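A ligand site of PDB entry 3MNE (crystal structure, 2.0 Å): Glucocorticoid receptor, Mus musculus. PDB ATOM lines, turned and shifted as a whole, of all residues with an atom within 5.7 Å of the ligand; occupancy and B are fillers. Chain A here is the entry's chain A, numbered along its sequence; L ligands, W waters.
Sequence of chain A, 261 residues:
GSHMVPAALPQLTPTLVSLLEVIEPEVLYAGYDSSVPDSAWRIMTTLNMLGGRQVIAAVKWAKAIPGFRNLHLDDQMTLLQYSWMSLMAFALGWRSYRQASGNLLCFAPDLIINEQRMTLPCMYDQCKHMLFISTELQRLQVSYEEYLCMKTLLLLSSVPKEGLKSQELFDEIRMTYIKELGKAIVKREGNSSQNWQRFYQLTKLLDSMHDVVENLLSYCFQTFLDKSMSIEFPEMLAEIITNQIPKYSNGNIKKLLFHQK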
ATOM      1  N   MET A  44       4.544 -14.874 -13.871  1.00  0.00           N
ATOM      2  CA  MET A  44       4.400 -13.430 -13.992  1.00  0.00           C
ATOM      3  C   MET A  44       5.707 -12.659 -13.965  1.00  0.00           C
ATOM      4  O   MET A  44       5.953 -11.793 -14.822  1.00  0.00           O
ATOM      5  CB  MET A  44       3.385 -12.866 -12.991  1.00  0.00           C
ATOM      6  CG  MET A  44       1.965 -13.207 -13.365  1.00  0.00           C
ATOM      7  SD  MET A  44       0.736 -13.008 -12.022  1.00  0.00           S
ATOM      8  CE  MET A  44       0.405 -11.486 -12.203  1.00  0.00           C
ATOM      9  N   THR A  45       6.520 -12.926 -12.957  1.00  0.00           N
ATOM     10  CA  THR A  45       7.813 -12.279 -12.846  1.00  0.00           C
ATOM     11  C   THR A  45       8.674 -12.519 -14.088  1.00  0.00           C
ATOM     12  O   THR A  45       9.322 -11.602 -14.587  1.00  0.00           O
ATOM     13  CB  THR A  45       8.527 -12.751 -11.593  1.00  0.00           C
ATOM     14  OG1 THR A  45       7.924 -12.124 -10.464  1.00  0.00           O
ATOM     15  CG2 THR A  45      10.019 -12.424 -11.652  1.00  0.00           C
ATOM     16  N   LEU A  47       7.628 -13.249 -17.127  1.00  0.00           N
ATOM     17  CA  LEU A  47       7.070 -12.507 -18.271  1.00  0.00           C
ATOM     18  C   LEU A  47       7.500 -11.053 -18.219  1.00  0.00           C
ATOM     19  O   LEU A  47       7.900 -10.498 -19.236  1.00  0.00           O
ATOM     20  CB  LEU A  47       5.549 -12.617 -18.320  1.00  0.00           C
ATOM     21  CG  LEU A  47       4.997 -14.018 -18.386  1.00  0.00           C
ATOM     22  CD1 LEU A  47       3.487 -13.892 -18.527  1.00  0.00           C
ATOM     23  CD2 LEU A  47       5.587 -14.811 -19.554  1.00  0.00           C
ATOM     24  N   ASN A  48       7.455 -10.461 -17.023  1.00  0.00           N
ATOM     25  CA  ASN A  48       7.861  -9.065 -16.847  1.00  0.00           C
ATOM     26  C   ASN A  48       9.329  -8.850 -17.231  1.00  0.00           C
ATOM     27  O   ASN A  48       9.665  -7.798 -17.813  1.00  0.00           O
ATOM     28  CB  ASN A  48       7.648  -8.581 -15.393  1.00  0.00           C
ATOM     29  CG  ASN A  48       6.178  -8.388 -15.045  1.00  0.00           C
ATOM     30  OD1 ASN A  48       5.374  -8.064 -15.912  1.00  0.00           O
ATOM     31  ND2 ASN A  48       5.816  -8.641 -13.786  1.00  0.00           N
ATOM     32  N   LEU A  50      11.108 -10.554 -19.330  1.00  0.00           N
ATOM     33  CA  LEU A  50      11.172 -10.580 -20.790  1.00  0.00           C
ATOM     34  C   LEU A  50      10.635  -9.284 -21.354  1.00  0.00           C
ATOM     35  O   LEU A  50      11.227  -8.676 -22.253  1.00  0.00           O
ATOM     36  CB  LEU A  50      10.358 -11.751 -21.362  1.00  0.00           C
ATOM     37  CG  LEU A  50      10.330 -11.893 -22.910  1.00  0.00           C
ATOM     38  CD1 LEU A  50      11.738 -12.209 -23.498  1.00  0.00           C
ATOM     39  CD2 LEU A  50       9.352 -13.023 -23.324  1.00  0.00           C
ATOM     40  N   GLY A  51       9.499  -8.840 -20.825  1.00  0.00           N
ATOM     41  CA  GLY A  51       8.845  -7.638 -21.293  1.00  0.00           C
ATOM     42  C   GLY A  51       9.711  -6.406 -21.240  1.00  0.00           C
ATOM     43  O   GLY A  51       9.640  -5.546 -22.122  1.00  0.00           O
ATOM     44  N   GLN A  54      11.948  -6.465 -24.225  1.00  0.00           N
ATOM     45  CA  GLN A  54      11.169  -6.208 -25.450  1.00  0.00           C
ATOM     46  C   GLN A  54      10.823  -4.740 -25.569  1.00  0.00           C
ATOM     47  O   GLN A  54      10.783  -4.194 -26.668  1.00  0.00           O
ATOM     48  CB  GLN A  54       9.883  -7.031 -25.444  1.00  0.00           C
ATOM     49  CG  GLN A  54      10.109  -8.489 -25.797  1.00  0.00           C
ATOM     50  CD  GLN A  54       8.850  -9.270 -25.580  1.00  0.00           C
ATOM     51  OE1 GLN A  54       7.861  -8.746 -25.082  1.00  0.00           O
ATOM     52  NE2 GLN A  54       8.830 -10.496 -26.051  1.00  0.00           N
ATOM     53  N   VAL A  55      10.616  -4.089 -24.441  1.00  0.00           N
ATOM     54  CA  VAL A  55      10.279  -2.661 -24.462  1.00  0.00           C
ATOM     55  C   VAL A  55      11.491  -1.806 -24.850  1.00  0.00           C
ATOM     56  O   VAL A  55      11.341  -0.787 -25.533  1.00  0.00           O
ATOM     57  CB  VAL A  55       9.574  -2.225 -23.140  1.00  0.00           C
ATOM     58  CG1 VAL A  55       9.478  -0.708 -23.032  1.00  0.00           C
ATOM     59  CG2 VAL A  55       8.153  -2.822 -23.093  1.00  0.00           C
ATOM     60  N   TRP A  84       3.064   1.325 -25.023  1.00  0.00           N
ATOM     61  CA  TRP A  84       3.900   0.100 -24.883  1.00  0.00           C
ATOM     62  C   TRP A  84       3.113  -1.228 -24.656  1.00  0.00           C
ATOM     63  O   TRP A  84       3.420  -2.241 -25.259  1.00  0.00           O
ATOM     64  CB  TRP A  84       5.025   0.273 -23.823  1.00  0.00           C
ATOM     65  CG  TRP A  84       4.512   0.172 -22.411  1.00  0.00           C
ATOM     66  CD1 TRP A  84       3.981   1.194 -21.643  1.00  0.00           C
ATOM     67  CD2 TRP A  84       4.359  -1.021 -21.633  1.00  0.00           C
ATOM     68  NE1 TRP A  84       3.562   0.711 -20.442  1.00  0.00           N
ATOM     69  CE2 TRP A  84       3.826  -0.638 -20.379  1.00  0.00           C
ATOM     70  CE3 TRP A  84       4.721  -2.361 -21.831  1.00  0.00           C
ATOM     71  CZ2 TRP A  84       3.590  -1.545 -19.353  1.00  0.00           C
ATOM     72  CZ3 TRP A  84       4.488  -3.256 -20.811  1.00  0.00           C
ATOM     73  CH2 TRP A  84       3.900  -2.846 -19.591  1.00  0.00           C
ATOM     74  N   MET A  85       2.116  -1.225 -23.774  1.00  0.00           N
ATOM     75  CA  MET A  85       1.396  -2.482 -23.523  1.00  0.00           C
ATOM     76  C   MET A  85       0.728  -2.945 -24.802  1.00  0.00           C
ATOM     77  O   MET A  85       0.700  -4.145 -25.106  1.00  0.00           O
ATOM     78  CB  MET A  85       0.353  -2.304 -22.398  1.00  0.00           C
ATOM     79  CG  MET A  85      -0.421  -3.603 -22.037  1.00  0.00           C
ATOM     80  SD  MET A  85       0.642  -4.946 -21.471  1.00  0.00           S
ATOM     81  CE  MET A  85       0.856  -4.519 -19.756  1.00  0.00           C
ATOM     82  N   MET A  88       3.421  -4.433 -27.141  1.00  0.00           N
ATOM     83  CA  MET A  88       3.859  -5.751 -26.644  1.00  0.00           C
ATOM     84  C   MET A  88       2.791  -6.841 -26.811  1.00  0.00           C
ATOM     85  O   MET A  88       3.090  -7.952 -27.220  1.00  0.00           O
ATOM     86  CB  MET A  88       4.251  -5.705 -25.163  1.00  0.00           C
ATOM     87  CG  MET A  88       5.414  -4.772 -24.806  1.00  0.00           C
ATOM     88  SD  MET A  88       6.870  -5.107 -25.833  1.00  0.00           S
ATOM     89  CE  MET A  88       6.745  -3.947 -27.062  1.00  0.00           C
ATOM     90  N   ALA A  89       1.555  -6.515 -26.466  1.00  0.00           N
ATOM     91  CA  ALA A  89       0.459  -7.485 -26.589  1.00  0.00           C
ATOM     92  C   ALA A  89       0.116  -7.844 -28.037  1.00  0.00           C
ATOM     93  O   ALA A  89      -0.156  -9.008 -28.349  1.00  0.00           O
ATOM     94  CB  ALA A  89      -0.782  -6.995 -25.851  1.00  0.00           C
ATOM     95  N   LEU A  92       2.880 -10.149 -29.247  1.00  0.00           N
ATOM     96  CA  LEU A  92       2.621 -11.460 -28.625  1.00  0.00           C
ATOM     97  C   LEU A  92       1.513 -12.207 -29.405  1.00  0.00           C
ATOM     98  O   LEU A  92       1.625 -13.398 -29.691  1.00  0.00           O
ATOM     99  CB  LEU A  92       2.228 -11.308 -27.134  1.00  0.00           C
ATOM    100  CG  LEU A  92       1.690 -12.553 -26.390  1.00  0.00           C
ATOM    101  CD1 LEU A  92       2.809 -13.669 -26.335  1.00  0.00           C
ATOM    102  CD2 LEU A  92       1.240 -12.140 -24.971  1.00  0.00           C
ATOM    103  N   ARG A  95       3.105 -13.536 -32.784  1.00  0.00           N
ATOM    104  CA  ARG A  95       3.959 -14.714 -32.625  1.00  0.00           C
ATOM    105  C   ARG A  95       3.119 -15.948 -32.309  1.00  0.00           C
ATOM    106  O   ARG A  95       3.410 -17.036 -32.799  1.00  0.00           O
ATOM    107  CB  ARG A  95       4.990 -14.500 -31.500  1.00  0.00           C
ATOM    108  CG  ARG A  95       6.005 -13.454 -31.876  1.00  0.00           C
ATOM    109  CD  ARG A  95       7.118 -13.320 -30.834  1.00  0.00           C
ATOM    110  NE  ARG A  95       6.630 -13.144 -29.460  1.00  0.00           N
ATOM    111  CZ  ARG A  95       6.454 -11.976 -28.862  1.00  0.00           C
ATOM    112  NH1 ARG A  95       6.623 -10.844 -29.534  1.00  0.00           N
ATOM    113  NH2 ARG A  95       6.094 -11.941 -27.588  1.00  0.00           N
ATOM    114  N   PHE A 107       5.367 -16.322 -26.002  1.00  0.00           N
ATOM    115  CA  PHE A 107       6.088 -15.182 -25.482  1.00  0.00           C
ATOM    116  C   PHE A 107       7.468 -15.043 -26.106  1.00  0.00           C
ATOM    117  O   PHE A 107       7.933 -13.918 -26.344  1.00  0.00           O
ATOM    118  CB  PHE A 107       6.185 -15.244 -23.933  1.00  0.00           C
ATOM    119  CG  PHE A 107       4.879 -14.968 -23.240  1.00  0.00           C
ATOM    120  CD1 PHE A 107       3.974 -16.002 -22.990  1.00  0.00           C
ATOM    121  CD2 PHE A 107       4.485 -13.649 -22.941  1.00  0.00           C
ATOM    122  CE1 PHE A 107       2.721 -15.733 -22.424  1.00  0.00           C
ATOM    123  CE2 PHE A 107       3.269 -13.366 -22.395  1.00  0.00           C
ATOM    124  CZ  PHE A 107       2.373 -14.397 -22.136  1.00  0.00           C
ATOM    125  N   GLN A 126      -5.859 -13.587 -16.993  1.00  0.00           N
ATOM    126  CA  GLN A 126      -4.949 -12.710 -17.729  1.00  0.00           C
ATOM    127  C   GLN A 126      -4.572 -13.293 -19.115  1.00  0.00           C
ATOM    128  O   GLN A 126      -4.439 -12.562 -20.086  1.00  0.00           O
ATOM    129  CB  GLN A 126      -3.733 -12.339 -16.916  1.00  0.00           C
ATOM    130  CG  GLN A 126      -2.892 -13.464 -16.374  1.00  0.00           C
ATOM    131  CD  GLN A 126      -1.898 -12.999 -15.287  1.00  0.00           C
ATOM    132  OE1 GLN A 126      -1.007 -12.189 -15.548  1.00  0.00           O
ATOM    133  NE2 GLN A 126      -2.020 -13.573 -14.095  1.00  0.00           N
ATOM    134  N   MET A 130      -4.808 -11.983 -23.648  1.00  0.00           N
ATOM    135  CA  MET A 130      -3.684 -12.079 -24.602  1.00  0.00           C
ATOM    136  C   MET A 130      -3.993 -13.019 -25.744  1.00  0.00           C
ATOM    137  O   MET A 130      -3.613 -12.792 -26.889  1.00  0.00           O
ATOM    138  CB  MET A 130      -2.454 -12.577 -23.873  1.00  0.00           C
ATOM    139  CG  MET A 130      -2.139 -11.779 -22.642  1.00  0.00           C
ATOM    140  SD  MET A 130      -0.677 -12.403 -21.865  1.00  0.00           S
ATOM    141  CE  MET A 130      -0.834 -11.863 -20.268  1.00  0.00           C
ATOM    142  N   ASN A 215      -7.695  -4.285 -20.090  1.00  0.00           N
ATOM    143  CA  ASN A 215      -7.696  -5.510 -19.261  1.00  0.00           C
ATOM    144  C   ASN A 215      -6.292  -5.863 -18.797  1.00  0.00           C
ATOM    145  O   ASN A 215      -6.071  -6.178 -17.632  1.00  0.00           O
ATOM    146  CB  ASN A 215      -8.314  -6.666 -20.070  1.00  0.00           C
ATOM    147  CG  ASN A 215      -9.811  -6.529 -20.186  1.00  0.00           C
ATOM    148  OD1 ASN A 215     -10.504  -6.526 -19.203  1.00  0.00           O
ATOM    149  ND2 ASN A 215     -10.306  -6.478 -21.394  1.00  0.00           N
ATOM    150  N   LEU A 216      -5.316  -5.752 -19.691  1.00  0.00           N
ATOM    151  CA  LEU A 216      -3.929  -6.044 -19.332  1.00  0.00           C
ATOM    152  C   LEU A 216      -3.300  -5.036 -18.354  1.00  0.00           C
ATOM    153  O   LEU A 216      -2.523  -5.432 -17.478  1.00  0.00           O
ATOM    154  CB  LEU A 216      -3.062  -6.165 -20.594  1.00  0.00           C
ATOM    155  CG  LEU A 216      -3.614  -7.249 -21.576  1.00  0.00           C
ATOM    156  CD1 LEU A 216      -2.812  -7.371 -22.897  1.00  0.00           C
ATOM    157  CD2 LEU A 216      -3.683  -8.641 -20.887  1.00  0.00           C
ATOM    158  N   TYR A 219      -4.032  -5.601 -14.646  1.00  0.00           N
ATOM    159  CA  TYR A 219      -3.107  -6.564 -14.012  1.00  0.00           C
ATOM    160  C   TYR A 219      -1.740  -5.937 -13.847  1.00  0.00           C
ATOM    161  O   TYR A 219      -1.122  -5.998 -12.784  1.00  0.00           O
ATOM    162  CB  TYR A 219      -2.981  -7.831 -14.891  1.00  0.00           C
ATOM    163  CG  TYR A 219      -4.082  -8.802 -14.593  1.00  0.00           C
ATOM    164  CD1 TYR A 219      -4.016  -9.590 -13.458  1.00  0.00           C
ATOM    165  CD2 TYR A 219      -5.221  -8.861 -15.373  1.00  0.00           C
ATOM    166  CE1 TYR A 219      -5.041 -10.457 -13.135  1.00  0.00           C
ATOM    167  CE2 TYR A 219      -6.259  -9.732 -15.046  1.00  0.00           C
ATOM    168  CZ  TYR A 219      -6.146 -10.520 -13.907  1.00  0.00           C
ATOM    169  OH  TYR A 219      -7.162 -11.346 -13.502  1.00  0.00           O
ATOM    170  N   CYS A 220      -1.242  -5.309 -14.913  1.00  0.00           N
ATOM    171  CA  CYS A 220       0.088  -4.697 -14.851  1.00  0.00           C
ATOM    172  C   CYS A 220       0.243  -3.755 -13.665  1.00  0.00           C
ATOM    173  O   CYS A 220       1.173  -3.881 -12.863  1.00  0.00           O
ATOM    174  CB  CYS A 220       0.406  -3.935 -16.156  1.00  0.00           C
ATOM    175  SG  CYS A 220       2.102  -3.300 -16.167  1.00  0.00           S
ATOM    176  N   PHE A 221      -0.677  -2.815 -13.550  1.00  0.00           N
ATOM    177  CA  PHE A 221      -0.613  -1.790 -12.524  1.00  0.00           C
ATOM    178  C   PHE A 221      -0.809  -2.338 -11.088  1.00  0.00           C
ATOM    179  O   PHE A 221      -0.124  -1.909 -10.169  1.00  0.00           O
ATOM    180  CB  PHE A 221      -1.682  -0.699 -12.800  1.00  0.00           C
ATOM    181  CG  PHE A 221      -1.427   0.146 -14.055  1.00  0.00           C
ATOM    182  CD1 PHE A 221      -0.194   0.099 -14.721  1.00  0.00           C
ATOM    183  CD2 PHE A 221      -2.435   0.954 -14.557  1.00  0.00           C
ATOM    184  CE1 PHE A 221      -0.011   0.818 -15.906  1.00  0.00           C
ATOM    185  CE2 PHE A 221      -2.260   1.707 -15.744  1.00  0.00           C
ATOM    186  CZ  PHE A 221      -1.044   1.669 -16.385  1.00  0.00           C
ATOM    187  N   THR A 223      -0.358  -5.522 -10.000  1.00  0.00           N
ATOM    188  CA  THR A 223       0.788  -6.356  -9.611  1.00  0.00           C
ATOM    189  C   THR A 223       2.030  -5.519  -9.381  1.00  0.00           C
ATOM    190  O   THR A 223       2.872  -5.878  -8.563  1.00  0.00           O
ATOM    191  CB  THR A 223       1.087  -7.536 -10.601  1.00  0.00           C
ATOM    192  OG1 THR A 223       1.430  -6.998 -11.886  1.00  0.00           O
ATOM    193  CG2 THR A 223      -0.124  -8.473 -10.729  1.00  0.00           C
ATOM    194  N   ILE A 231       5.836  -9.625  -7.000  1.00  0.00           N
ATOM    195  CA  ILE A 231       5.967  -9.884  -8.437  1.00  0.00           C
ATOM    196  C   ILE A 231       6.944  -8.832  -8.880  1.00  0.00           C
ATOM    197  O   ILE A 231       6.752  -7.650  -8.614  1.00  0.00           O
ATOM    198  CB  ILE A 231       4.614  -9.759  -9.166  1.00  0.00           C
ATOM    199  CG1 ILE A 231       3.795 -11.047  -8.939  1.00  0.00           C
ATOM    200  CG2 ILE A 231       4.838  -9.520 -10.704  1.00  0.00           C
ATOM    201  CD1 ILE A 231       2.299 -10.850  -9.034  1.00  0.00           C
ATOM    202  N   PHE A 233       9.441  -6.573 -11.506  1.00  0.00           N
ATOM    203  CA  PHE A 233       9.529  -5.895 -12.808  1.00  0.00           C
ATOM    204  C   PHE A 233      10.934  -5.343 -12.961  1.00  0.00           C
ATOM    205  O   PHE A 233      11.472  -4.740 -12.026  1.00  0.00           O
ATOM    206  CB  PHE A 233       8.584  -4.690 -12.851  1.00  0.00           C
ATOM    207  CG  PHE A 233       7.126  -5.039 -12.893  1.00  0.00           C
ATOM    208  CD1 PHE A 233       6.492  -5.488 -11.750  1.00  0.00           C
ATOM    209  CD2 PHE A 233       6.414  -4.955 -14.073  1.00  0.00           C
ATOM    210  CE1 PHE A 233       5.147  -5.828 -11.786  1.00  0.00           C
ATOM    211  CE2 PHE A 233       5.058  -5.268 -14.126  1.00  0.00           C
ATOM    212  CZ  PHE A 233       4.429  -5.685 -12.967  1.00  0.00           C
ATOM    213  N   LEU A 237      10.900  -1.164 -17.322  1.00  0.00           N
ATOM    214  CA  LEU A 237       9.454  -1.301 -17.223  1.00  0.00           C
ATOM    215  C   LEU A 237       8.957  -0.559 -15.989  1.00  0.00           C
ATOM    216  O   LEU A 237       7.954   0.168 -16.046  1.00  0.00           O
ATOM    217  CB  LEU A 237       9.083  -2.785 -17.108  1.00  0.00           C
ATOM    218  CG  LEU A 237       7.966  -3.246 -18.028  1.00  0.00           C
ATOM    219  CD1 LEU A 237       8.048  -2.517 -19.360  1.00  0.00           C
ATOM    220  CD2 LEU A 237       7.962  -4.760 -18.189  1.00  0.00           C
HETATM  221  C1  LIG L   1       5.825  -9.326 -21.612  1.00  0.00           C
HETATM  222  C2  LIG L   1       6.346 -10.062 -22.644  1.00  0.00           C
HETATM  223  C3  LIG L   1       5.478 -10.179 -23.883  1.00  0.00           C
HETATM  224  C4  LIG L   1       4.131  -9.531 -24.007  1.00  0.00           C
HETATM  225  C5  LIG L   1       3.635  -8.781 -22.954  1.00  0.00           C
HETATM  226  C6  LIG L   1       2.230  -8.100 -23.071  1.00  0.00           C
HETATM  227  C7  LIG L   1       1.362  -8.623 -21.831  1.00  0.00           C
HETATM  228  C8  LIG L   1       2.209  -8.438 -20.445  1.00  0.00           C
HETATM  229  C9  LIG L   1       3.644  -9.223 -20.401  1.00  0.00           C
HETATM  230  C10 LIG L   1       4.445  -8.616 -21.650  1.00  0.00           C
HETATM  231  C11 LIG L   1       4.471  -9.229 -19.041  1.00  0.00           C
HETATM  232  C12 LIG L   1       3.470  -9.504 -17.811  1.00  0.00           C
HETATM  233  C13 LIG L   1       2.058  -8.719 -17.951  1.00  0.00           C
HETATM  234  C14 LIG L   1       1.300  -9.026 -19.236  1.00  0.00           C
HETATM  235  C15 LIG L   1      -0.054  -8.263 -19.180  1.00  0.00           C
HETATM  236  C16 LIG L   1      -0.369  -8.560 -17.634  1.00  0.00           C
HETATM  237  C17 LIG L   1       0.914  -9.314 -17.038  1.00  0.00           C
HETATM  238  C18 LIG L   1       2.511  -7.306 -17.465  1.00  0.00           C
HETATM  239  C19 LIG L   1       4.815  -7.069 -21.605  1.00  0.00           C
HETATM  240  C20 LIG L   1       1.250  -8.942 -15.556  1.00  0.00           C
HETATM  241  C21 LIG L   1       1.975  -9.864 -14.613  1.00  0.00           C
HETATM  242  C22 LIG L   1      -1.517  -9.533 -17.392  1.00  0.00           C
HETATM  243  F1  LIG L   1       3.185 -10.553 -20.750  1.00  0.00           F
HETATM  244  O1  LIG L   1       5.900 -10.833 -24.836  1.00  0.00           O
HETATM  245  O2  LIG L   1       4.961  -7.898 -18.692  1.00  0.00           O
HETATM  246  O3  LIG L   1       0.826 -10.796 -17.009  1.00  0.00           O
HETATM  247  O4  LIG L   1       0.593  -8.043 -14.963  1.00  0.00           O
HETATM  248  O5  LIG L   1       2.658  -9.055 -13.600  1.00  0.00           O
HETATM  249  O   HOH W   1       5.805  -8.797 -27.315  1.00  0.00           O
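The guanidinium group (NH2) of Arg 95 sits at hydrogen-bond distance from an oxygen (O1) of the ligand, at 3.0 Å. The side-chain amide oxygen (OD1) of Asn 48 is in hydrogen-bond range of an oxygen (O2) of the ligand (2.8 Å). The side-chain hydroxyl of Thr 223 lies within hydrogen-bond range of an oxygen (O5) of the ligand (2.9 Å). O1 of the ligand lies close to OE1 of Gln 54 (2.9 Å). O3 of the ligand lies within hydrogen-bond range of OE1 of Gln 126, at 2.7 Å. O4 of the ligand lies within hydrogen-bond range of N of Cys 220 (3.3 Å).
O of Cys 220 lies within hydrogen-bond range of OG1 of Thr 223 (3.3 Å). The backbone carbonyl oxygen (O) of Tyr 219 sits at hydrogen-bond distance from the side-chain hydroxyl (OG1) of Thr 223 (2.9 Å). The side-chain sulfur (SD) of Met 44 lies within hydrogen-bond range of the side-chain amide nitrogen (NE2) of Gln 126 (3.5 Å). The guanidinium group (NH2) of Arg 95 is in hydrogen-bond range of the backbone carbonyl oxygen (O) of Phe 107, 3.0 Å away. NH2 of Arg 95 sits close to NE2 of Gln 54, at 3.5 Å. The side-chain amide nitrogen (ND2) of Asn 48 sits at hydrogen-bond distance from the backbone carbonyl oxygen (O) of Met 44, at 3.3 Å.
The backbone carbonyl oxygen (O) of Tyr 219 sits close to an oxygen (O4) of the ligand (3.4 Å). Merely in contact with the ligand: Met 44 (3.3 Å), Leu 47 (3.4 Å), Gly 51 (3.5 Å), Trp 84 (3.9 Å), Met 85 (3.8 Å), Met 88 (3.7 Å), Ala 89 (3.8 Å), Phe 107 (3.3 Å), Met 130 (3.7 Å), Leu 216 (3.8 Å), Ile 231 (3.7 Å) and Phe 233 (3.9 Å). Hydrophobic or aromatic side chains that line the ligand: Met 44, Leu 47, Trp 84, Met 85, Met 88, Phe 107, Met 130, Leu 216, Tyr 219, Ile 231 and Phe 233. Of the 26 residues printed, 19 come within 4 Å of the ligand.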
